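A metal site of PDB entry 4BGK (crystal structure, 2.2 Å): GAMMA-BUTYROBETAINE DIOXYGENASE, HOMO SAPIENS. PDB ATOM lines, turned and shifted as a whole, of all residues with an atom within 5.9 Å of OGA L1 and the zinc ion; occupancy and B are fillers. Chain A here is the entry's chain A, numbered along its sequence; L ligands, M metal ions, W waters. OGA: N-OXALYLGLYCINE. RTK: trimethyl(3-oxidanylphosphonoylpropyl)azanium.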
ATOM      1  N   TRP A 181       8.887  23.691   6.058  1.00  0.00           N
ATOM      2  CA  TRP A 181       9.848  23.449   7.149  1.00  0.00           C
ATOM      3  C   TRP A 181      11.130  24.207   6.894  1.00  0.00           C
ATOM      4  O   TRP A 181      11.457  24.549   5.744  1.00  0.00           O
ATOM      5  CB  TRP A 181      10.147  21.965   7.343  1.00  0.00           C
ATOM      6  CG  TRP A 181       9.928  21.122   6.133  1.00  0.00           C
ATOM      7  CD1 TRP A 181       8.799  20.488   5.789  1.00  0.00           C
ATOM      8  CD2 TRP A 181      10.878  20.833   5.095  1.00  0.00           C
ATOM      9  NE1 TRP A 181       8.962  19.833   4.598  1.00  0.00           N
ATOM     10  CE2 TRP A 181      10.237  20.021   4.146  1.00  0.00           C
ATOM     11  CE3 TRP A 181      12.216  21.192   4.879  1.00  0.00           C
ATOM     12  CZ2 TRP A 181      10.860  19.561   3.013  1.00  0.00           C
ATOM     13  CZ3 TRP A 181      12.828  20.730   3.755  1.00  0.00           C
ATOM     14  CH2 TRP A 181      12.162  19.924   2.833  1.00  0.00           C
ATOM     15  N   VAL A 183      15.094  24.529   7.008  1.00  0.00           N
ATOM     16  CA  VAL A 183      16.371  23.833   7.071  1.00  0.00           C
ATOM     17  C   VAL A 183      17.397  24.816   7.607  1.00  0.00           C
ATOM     18  O   VAL A 183      17.818  25.742   6.916  1.00  0.00           O
ATOM     19  CB  VAL A 183      16.829  23.297   5.703  1.00  0.00           C
ATOM     20  CG1 VAL A 183      18.088  22.460   5.867  1.00  0.00           C
ATOM     21  CG2 VAL A 183      15.701  22.513   5.059  1.00  0.00           C
ATOM     22  N   ASN A 191      16.474  16.069  13.472  1.00  0.00           N
ATOM     23  CA  ASN A 191      16.800  15.540  12.139  1.00  0.00           C
ATOM     24  C   ASN A 191      18.178  16.020  11.766  1.00  0.00           C
ATOM     25  O   ASN A 191      18.528  17.154  12.070  1.00  0.00           O
ATOM     26  CB  ASN A 191      15.764  16.010  11.122  1.00  0.00           C
ATOM     27  CG  ASN A 191      15.827  15.238   9.807  1.00  0.00           C
ATOM     28  OD1 ASN A 191      16.650  15.518   8.942  1.00  0.00           O
ATOM     29  ND2 ASN A 191      14.903  14.295   9.633  1.00  0.00           N
ATOM     30  N   ALA A 193      19.296  16.889   9.060  1.00  0.00           N
ATOM     31  CA  ALA A 193      19.191  18.023   8.149  1.00  0.00           C
ATOM     32  C   ALA A 193      19.264  19.346   8.890  1.00  0.00           C
ATOM     33  O   ALA A 193      19.731  20.355   8.348  1.00  0.00           O
ATOM     34  CB  ALA A 193      17.905  17.940   7.349  1.00  0.00           C
ATOM     35  N   TYR A 194      18.823  19.348  10.141  1.00  0.00           N
ATOM     36  CA  TYR A 194      18.762  20.584  10.923  1.00  0.00           C
ATOM     37  C   TYR A 194      20.006  20.707  11.816  1.00  0.00           C
ATOM     38  O   TYR A 194      19.909  21.085  12.986  1.00  0.00           O
ATOM     39  CB  TYR A 194      17.486  20.620  11.771  1.00  0.00           C
ATOM     40  CG  TYR A 194      16.165  20.468  11.013  1.00  0.00           C
ATOM     41  CD1 TYR A 194      16.015  20.912   9.688  1.00  0.00           C
ATOM     42  CD2 TYR A 194      15.053  19.930  11.644  1.00  0.00           C
ATOM     43  CE1 TYR A 194      14.810  20.795   9.021  1.00  0.00           C
ATOM     44  CE2 TYR A 194      13.831  19.798  10.987  1.00  0.00           C
ATOM     45  CZ  TYR A 194      13.727  20.226   9.678  1.00  0.00           C
ATOM     46  OH  TYR A 194      12.526  20.091   9.033  1.00  0.00           O
ATOM     47  N   LEU A 199      25.245  16.194   4.336  1.00  0.00           N
ATOM     48  CA  LEU A 199      24.266  15.213   3.977  1.00  0.00           C
ATOM     49  C   LEU A 199      24.789  14.564   2.726  1.00  0.00           C
ATOM     50  O   LEU A 199      25.004  15.234   1.708  1.00  0.00           O
ATOM     51  CB  LEU A 199      22.910  15.884   3.704  1.00  0.00           C
ATOM     52  CG  LEU A 199      22.367  16.647   4.903  1.00  0.00           C
ATOM     53  CD1 LEU A 199      21.075  17.346   4.534  1.00  0.00           C
ATOM     54  CD2 LEU A 199      22.153  15.722   6.073  1.00  0.00           C
ATOM     55  N   HIS A 202      20.933  11.218  -0.718  1.00  0.00           N
ATOM     56  CA  HIS A 202      19.785  10.545  -0.152  1.00  0.00           C
ATOM     57  C   HIS A 202      18.559  11.026  -0.858  1.00  0.00           C
ATOM     58  O   HIS A 202      18.561  12.099  -1.479  1.00  0.00           O
ATOM     59  CB  HIS A 202      19.669  10.883   1.353  1.00  0.00           C
ATOM     60  CG  HIS A 202      19.341  12.318   1.634  1.00  0.00           C
ATOM     61  ND1 HIS A 202      20.276  13.323   1.592  1.00  0.00           N
ATOM     62  CD2 HIS A 202      18.174  12.913   1.955  1.00  0.00           C
ATOM     63  CE1 HIS A 202      19.700  14.475   1.867  1.00  0.00           C
ATOM     64  NE2 HIS A 202      18.424  14.251   2.099  1.00  0.00           N
ATOM     65  N   THR A 203      17.499  10.241  -0.768  1.00  0.00           N
ATOM     66  CA  THR A 203      16.144  10.702  -1.033  1.00  0.00           C
ATOM     67  C   THR A 203      15.524  11.100   0.276  1.00  0.00           C
ATOM     68  O   THR A 203      15.935  10.607   1.323  1.00  0.00           O
ATOM     69  CB  THR A 203      15.269   9.612  -1.705  1.00  0.00           C
ATOM     70  OG1 THR A 203      15.065   8.475  -0.850  1.00  0.00           O
ATOM     71  CG2 THR A 203      15.909   9.148  -3.007  1.00  0.00           C
ATOM     72  N   ASP A 204      14.517  11.972   0.230  1.00  0.00           N
ATOM     73  CA  ASP A 204      13.795  12.390   1.436  1.00  0.00           C
ATOM     74  C   ASP A 204      12.645  11.441   1.792  1.00  0.00           C
ATOM     75  O   ASP A 204      11.926  10.971   0.907  1.00  0.00           O
ATOM     76  CB  ASP A 204      13.253  13.822   1.318  1.00  0.00           C
ATOM     77  CG  ASP A 204      14.232  14.853   1.855  1.00  0.00           C
ATOM     78  OD1 ASP A 204      15.421  14.596   1.762  1.00  0.00           O
ATOM     79  OD2 ASP A 204      13.809  15.910   2.367  1.00  0.00           O
ATOM     80  N   GLN A 215      10.137  17.648  -4.321  1.00  0.00           N
ATOM     81  CA  GLN A 215      10.609  18.409  -3.195  1.00  0.00           C
ATOM     82  C   GLN A 215      10.927  19.820  -3.686  1.00  0.00           C
ATOM     83  O   GLN A 215      11.433  20.003  -4.772  1.00  0.00           O
ATOM     84  CB  GLN A 215      11.862  17.743  -2.622  1.00  0.00           C
ATOM     85  CG  GLN A 215      12.508  18.522  -1.508  1.00  0.00           C
ATOM     86  CD  GLN A 215      13.505  17.701  -0.720  1.00  0.00           C
ATOM     87  OE1 GLN A 215      14.271  18.257   0.062  1.00  0.00           O
ATOM     88  NE2 GLN A 215      13.506  16.387  -0.928  1.00  0.00           N
ATOM     89  N   LEU A 217      12.941  23.422  -2.517  1.00  0.00           N
ATOM     90  CA  LEU A 217      13.880  24.049  -1.569  1.00  0.00           C
ATOM     91  C   LEU A 217      14.219  25.474  -1.997  1.00  0.00           C
ATOM     92  O   LEU A 217      14.723  25.737  -3.100  1.00  0.00           O
ATOM     93  CB  LEU A 217      15.174  23.248  -1.455  1.00  0.00           C
ATOM     94  CG  LEU A 217      15.168  21.956  -0.635  1.00  0.00           C
ATOM     95  CD1 LEU A 217      16.542  21.294  -0.704  1.00  0.00           C
ATOM     96  CD2 LEU A 217      14.806  22.224   0.806  1.00  0.00           C
ATOM     97  N   GLY A 227      28.037  24.313   2.375  1.00  0.00           N
ATOM     98  CA  GLY A 227      26.600  24.287   2.098  1.00  0.00           C
ATOM     99  C   GLY A 227      26.231  24.221   0.636  1.00  0.00           C
ATOM    100  O   GLY A 227      25.074  24.469   0.290  1.00  0.00           O
ATOM    101  N   ASP A 228      27.191  23.841  -0.211  1.00  0.00           N
ATOM    102  CA  ASP A 228      26.967  23.519  -1.615  1.00  0.00           C
ATOM    103  C   ASP A 228      25.998  22.361  -1.726  1.00  0.00           C
ATOM    104  O   ASP A 228      25.959  21.513  -0.875  1.00  0.00           O
ATOM    105  CB  ASP A 228      28.277  23.122  -2.319  1.00  0.00           C
ATOM    106  CG  ASP A 228      29.372  24.150  -2.122  1.00  0.00           C
ATOM    107  OD1 ASP A 228      29.926  24.231  -1.004  1.00  0.00           O
ATOM    108  OD2 ASP A 228      29.660  24.870  -3.076  1.00  0.00           O
ATOM    109  N   SER A 229      25.254  22.342  -2.812  1.00  0.00           N
ATOM    110  CA  SER A 229      24.324  21.280  -3.098  1.00  0.00           C
ATOM    111  C   SER A 229      24.957  20.327  -4.069  1.00  0.00           C
ATOM    112  O   SER A 229      25.824  20.689  -4.885  1.00  0.00           O
ATOM    113  CB  SER A 229      23.043  21.848  -3.717  1.00  0.00           C
ATOM    114  OG  SER A 229      22.477  22.875  -2.916  1.00  0.00           O
ATOM    115  N   ASN A 292      17.804   6.853   2.478  1.00  0.00           N
ATOM    116  CA  ASN A 292      18.418   7.854   3.318  1.00  0.00           C
ATOM    117  C   ASN A 292      19.206   7.143   4.416  1.00  0.00           C
ATOM    118  O   ASN A 292      18.641   6.409   5.237  1.00  0.00           O
ATOM    119  CB  ASN A 292      17.371   8.815   3.866  1.00  0.00           C
ATOM    120  CG  ASN A 292      17.987   9.958   4.665  1.00  0.00           C
ATOM    121  OD1 ASN A 292      19.168   9.890   5.061  1.00  0.00           O
ATOM    122  ND2 ASN A 292      17.195  10.993   4.934  1.00  0.00           N
ATOM    123  N   MET A 332      23.332  27.215  -4.032  1.00  0.00           N
ATOM    124  CA  MET A 332      22.131  28.024  -4.045  1.00  0.00           C
ATOM    125  C   MET A 332      22.420  29.413  -3.466  1.00  0.00           C
ATOM    126  O   MET A 332      23.172  29.514  -2.508  1.00  0.00           O
ATOM    127  CB  MET A 332      21.037  27.342  -3.240  1.00  0.00           C
ATOM    128  CG  MET A 332      20.470  26.102  -3.913  1.00  0.00           C
ATOM    129  SD  MET A 332      19.079  25.422  -2.971  1.00  0.00           S
ATOM    130  CE  MET A 332      17.791  26.541  -3.524  1.00  0.00           C
ATOM    131  N   HIS A 347      20.000  13.691  -3.459  1.00  0.00           N
ATOM    132  CA  HIS A 347      20.556  14.995  -3.216  1.00  0.00           C
ATOM    133  C   HIS A 347      21.301  15.048  -1.921  1.00  0.00           C
ATOM    134  O   HIS A 347      21.159  14.176  -1.019  1.00  0.00           O
ATOM    135  CB  HIS A 347      19.455  16.030  -3.245  1.00  0.00           C
ATOM    136  CG  HIS A 347      18.452  15.890  -2.159  1.00  0.00           C
ATOM    137  ND1 HIS A 347      17.524  14.865  -2.125  1.00  0.00           N
ATOM    138  CD2 HIS A 347      18.223  16.652  -1.055  1.00  0.00           C
ATOM    139  CE1 HIS A 347      16.771  15.008  -1.043  1.00  0.00           C
ATOM    140  NE2 HIS A 347      17.185  16.066  -0.382  1.00  0.00           N
ATOM    141  N   GLY A 348      22.164  16.047  -1.830  1.00  0.00           N
ATOM    142  CA  GLY A 348      22.956  16.219  -0.630  1.00  0.00           C
ATOM    143  C   GLY A 348      23.479  17.619  -0.469  1.00  0.00           C
ATOM    144  O   GLY A 348      23.193  18.523  -1.272  1.00  0.00           O
ATOM    145  N   ARG A 349      24.304  17.777   0.534  1.00  0.00           N
ATOM    146  CA  ARG A 349      24.783  19.084   0.909  1.00  0.00           C
ATOM    147  C   ARG A 349      26.148  18.946   1.595  1.00  0.00           C
ATOM    148  O   ARG A 349      26.358  18.043   2.419  1.00  0.00           O
ATOM    149  CB  ARG A 349      23.761  19.748   1.827  1.00  0.00           C
ATOM    150  CG  ARG A 349      24.357  20.681   2.852  1.00  0.00           C
ATOM    151  CD  ARG A 349      23.360  21.125   3.892  1.00  0.00           C
ATOM    152  NE  ARG A 349      23.535  20.474   5.177  1.00  0.00           N
ATOM    153  CZ  ARG A 349      22.569  20.335   6.085  1.00  0.00           C
ATOM    154  NH1 ARG A 349      21.342  20.785   5.845  1.00  0.00           N
ATOM    155  NH2 ARG A 349      22.842  19.718   7.227  1.00  0.00           N
ATOM    156  N   ARG A 360      22.582  30.197   7.539  1.00  0.00           N
ATOM    157  CA  ARG A 360      22.077  29.398   6.443  1.00  0.00           C
ATOM    158  C   ARG A 360      20.646  28.945   6.726  1.00  0.00           C
ATOM    159  O   ARG A 360      20.372  28.388   7.789  1.00  0.00           O
ATOM    160  CB  ARG A 360      22.947  28.169   6.199  1.00  0.00           C
ATOM    161  CG  ARG A 360      22.643  27.506   4.863  1.00  0.00           C
ATOM    162  CD  ARG A 360      23.495  26.296   4.645  1.00  0.00           C
ATOM    163  NE  ARG A 360      23.364  25.717   3.313  1.00  0.00           N
ATOM    164  CZ  ARG A 360      22.543  24.732   2.963  1.00  0.00           C
ATOM    165  NH1 ARG A 360      21.659  24.203   3.831  1.00  0.00           N
ATOM    166  NH2 ARG A 360      22.561  24.291   1.727  1.00  0.00           N
ATOM    167  N   LEU A 362      17.166  27.379   4.577  1.00  0.00           N
ATOM    168  CA  LEU A 362      16.289  27.046   3.472  1.00  0.00           C
ATOM    169  C   LEU A 362      14.868  26.801   3.982  1.00  0.00           C
ATOM    170  O   LEU A 362      14.676  26.426   5.141  1.00  0.00           O
ATOM    171  CB  LEU A 362      16.810  25.844   2.710  1.00  0.00           C
ATOM    172  CG  LEU A 362      18.292  25.682   2.431  1.00  0.00           C
ATOM    173  CD1 LEU A 362      18.502  24.359   1.693  1.00  0.00           C
ATOM    174  CD2 LEU A 362      18.885  26.835   1.630  1.00  0.00           C
ATOM    175  N   TYR A 366       7.028  19.613   0.239  1.00  0.00           N
ATOM    176  CA  TYR A 366       6.889  18.468  -0.614  1.00  0.00           C
ATOM    177  C   TYR A 366       5.605  18.592  -1.441  1.00  0.00           C
ATOM    178  O   TYR A 366       4.651  19.250  -1.019  1.00  0.00           O
ATOM    179  CB  TYR A 366       6.807  17.208   0.234  1.00  0.00           C
ATOM    180  CG  TYR A 366       8.057  16.893   1.042  1.00  0.00           C
ATOM    181  CD1 TYR A 366       9.301  16.726   0.402  1.00  0.00           C
ATOM    182  CD2 TYR A 366       7.999  16.772   2.418  1.00  0.00           C
ATOM    183  CE1 TYR A 366      10.439  16.421   1.135  1.00  0.00           C
ATOM    184  CE2 TYR A 366       9.122  16.484   3.148  1.00  0.00           C
ATOM    185  CZ  TYR A 366      10.333  16.285   2.507  1.00  0.00           C
ATOM    186  OH  TYR A 366      11.440  16.006   3.265  1.00  0.00           O
HETATM  187  C1  OGA L   1      17.044  18.120   3.446  1.00  0.00           C
HETATM  188  C2  OGA L   1      18.147  18.466   2.527  1.00  0.00           C
HETATM  189  C4  OGA L   1      19.623  20.119   1.527  1.00  0.00           C
HETATM  190  C5  OGA L   1      20.408  21.319   2.017  1.00  0.00           C
HETATM  191  O1  OGA L   1      16.689  18.946   4.339  1.00  0.00           O
HETATM  192  O2  OGA L   1      16.476  17.002   3.298  1.00  0.00           O
HETATM  193  O2' OGA L   1      18.528  17.628   1.740  1.00  0.00           O
HETATM  194  O3  OGA L   1      21.149  21.861   1.182  1.00  0.00           O
HETATM  195  N1  OGA L   1      18.664  19.690   2.540  1.00  0.00           N
HETATM  196  O4  OGA L   1      20.317  21.702   3.218  1.00  0.00           O
HETATM  197  O7  RTK L   2      14.397  11.452   5.065  1.00  0.00           O
HETATM  198  P5  RTK L   2      14.343  12.740   5.825  1.00  0.00           P
HETATM  199  O4  RTK L   2      14.550  12.542   7.319  1.00  0.00           O
HETATM  200  C6  RTK L   2      12.759  13.540   5.444  1.00  0.00           C
HETATM  201  C3  RTK L   2      12.541  14.789   6.288  1.00  0.00           C
HETATM  202  C2  RTK L   2      13.493  15.891   5.857  1.00  0.00           C
HETATM  203  N1  RTK L   2      13.261  17.217   6.491  1.00  0.00           N
HETATM  204  C28 RTK L   2      13.498  17.202   7.954  1.00  0.00           C
HETATM  205  C9  RTK L   2      11.908  17.741   6.220  1.00  0.00           C
HETATM  206  C8  RTK L   2      14.262  18.112   5.870  1.00  0.00           C
HETATM  207 ZN    ZN M   1      17.070  15.924   1.787  1.00  0.00          ZN
HETATM  208  O   HOH W   1      21.335  20.901  -1.184  1.00  0.00           O
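The backbone NH (N) of Leu 199 is in hydrogen-bond range of the backbone carbonyl oxygen (O) of Arg 349 (2.9 Å).
The guanidinium group of Arg 349 sits at hydrogen-bond distance from the backbone carbonyl oxygen of Ala 193 (3.0 Å).
The backbone NH (N) of Val 183 is in hydrogen-bond range of the backbone carbonyl oxygen (O) of Leu 362 (2.7 Å).
The guanidinium group of Arg 360 is in hydrogen-bond range of the backbone carbonyl oxygen of Gly 227 (2.9 Å).
The backbone NH (N) of Ala 193 sits at hydrogen-bond distance from the side-chain amide oxygen (OD1) of Asn 191.
The side-chain carboxylate (OD2) of Asp 204 lies close to the side-chain amide oxygen (OE1) of Gln 215 (3.3 Å).
The side-chain hydroxyl of Tyr 366 is in hydrogen-bond range of the side-chain carboxylate of Asp 204, at 2.5 Å.
The zinc ion is bound by O2 of OGA L1 (1.9 Å).
The side-chain carboxylate (OD1) of Asp 204 is bound to the zinc ion (2.1 Å).
The zinc ion is bound by NE2 of His 202 (2.2 Å).
A ring nitrogen (NE2) of His 347 binds the zinc ion.
An oxygen (O2') of OGA L1 binds the zinc ion (2.2 Å).
Water W1 lies within hydrogen-bond range of an oxygen (O3) of OGA L1 (2.6 Å), the side-chain hydroxyl (OG) of Ser 229 (2.9 Å) and the backbone carbonyl oxygen (O) of Gly 348 (3.0 Å).
Merely in contact with OGA L1: Val 183 (3.5 Å), Ala 193 (3.4 Å), Leu 199 (3.7 Å), Leu 217 (3.98 Å) and Leu 362 (3.6 Å).
Hydrophobic or aromatic side chains within 4 Å of OGA L1: Val 183, Ala 193, Leu 199, His 202, Leu 217, His 347 and Leu 362.
Within 4 Å of OGA L1: Val 183, Ala 193, Leu 199, His 202, Asp 204, Leu 217, His 347, Arg 349, Arg 360 and Leu 362.
The nearest printed residue that does not touch OGA L1 is Gln 215 (4.1 Å).
The side-chain amide nitrogen of Asn 191 sits at hydrogen-bond distance from an oxygen (O4) of RTK L2 (2.9 Å).
ND2 of Asn 292 lies within hydrogen-bond range of O7 of RTK L2 (2.8 Å).
NH1 of Arg 349 lies within salt-bridge range of O4 of OGA L1, 3.0 Å away.
An oxygen (O3) of OGA L1 is in salt-bridge range of the guanidinium group of Arg 360, at 2.9 Å.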
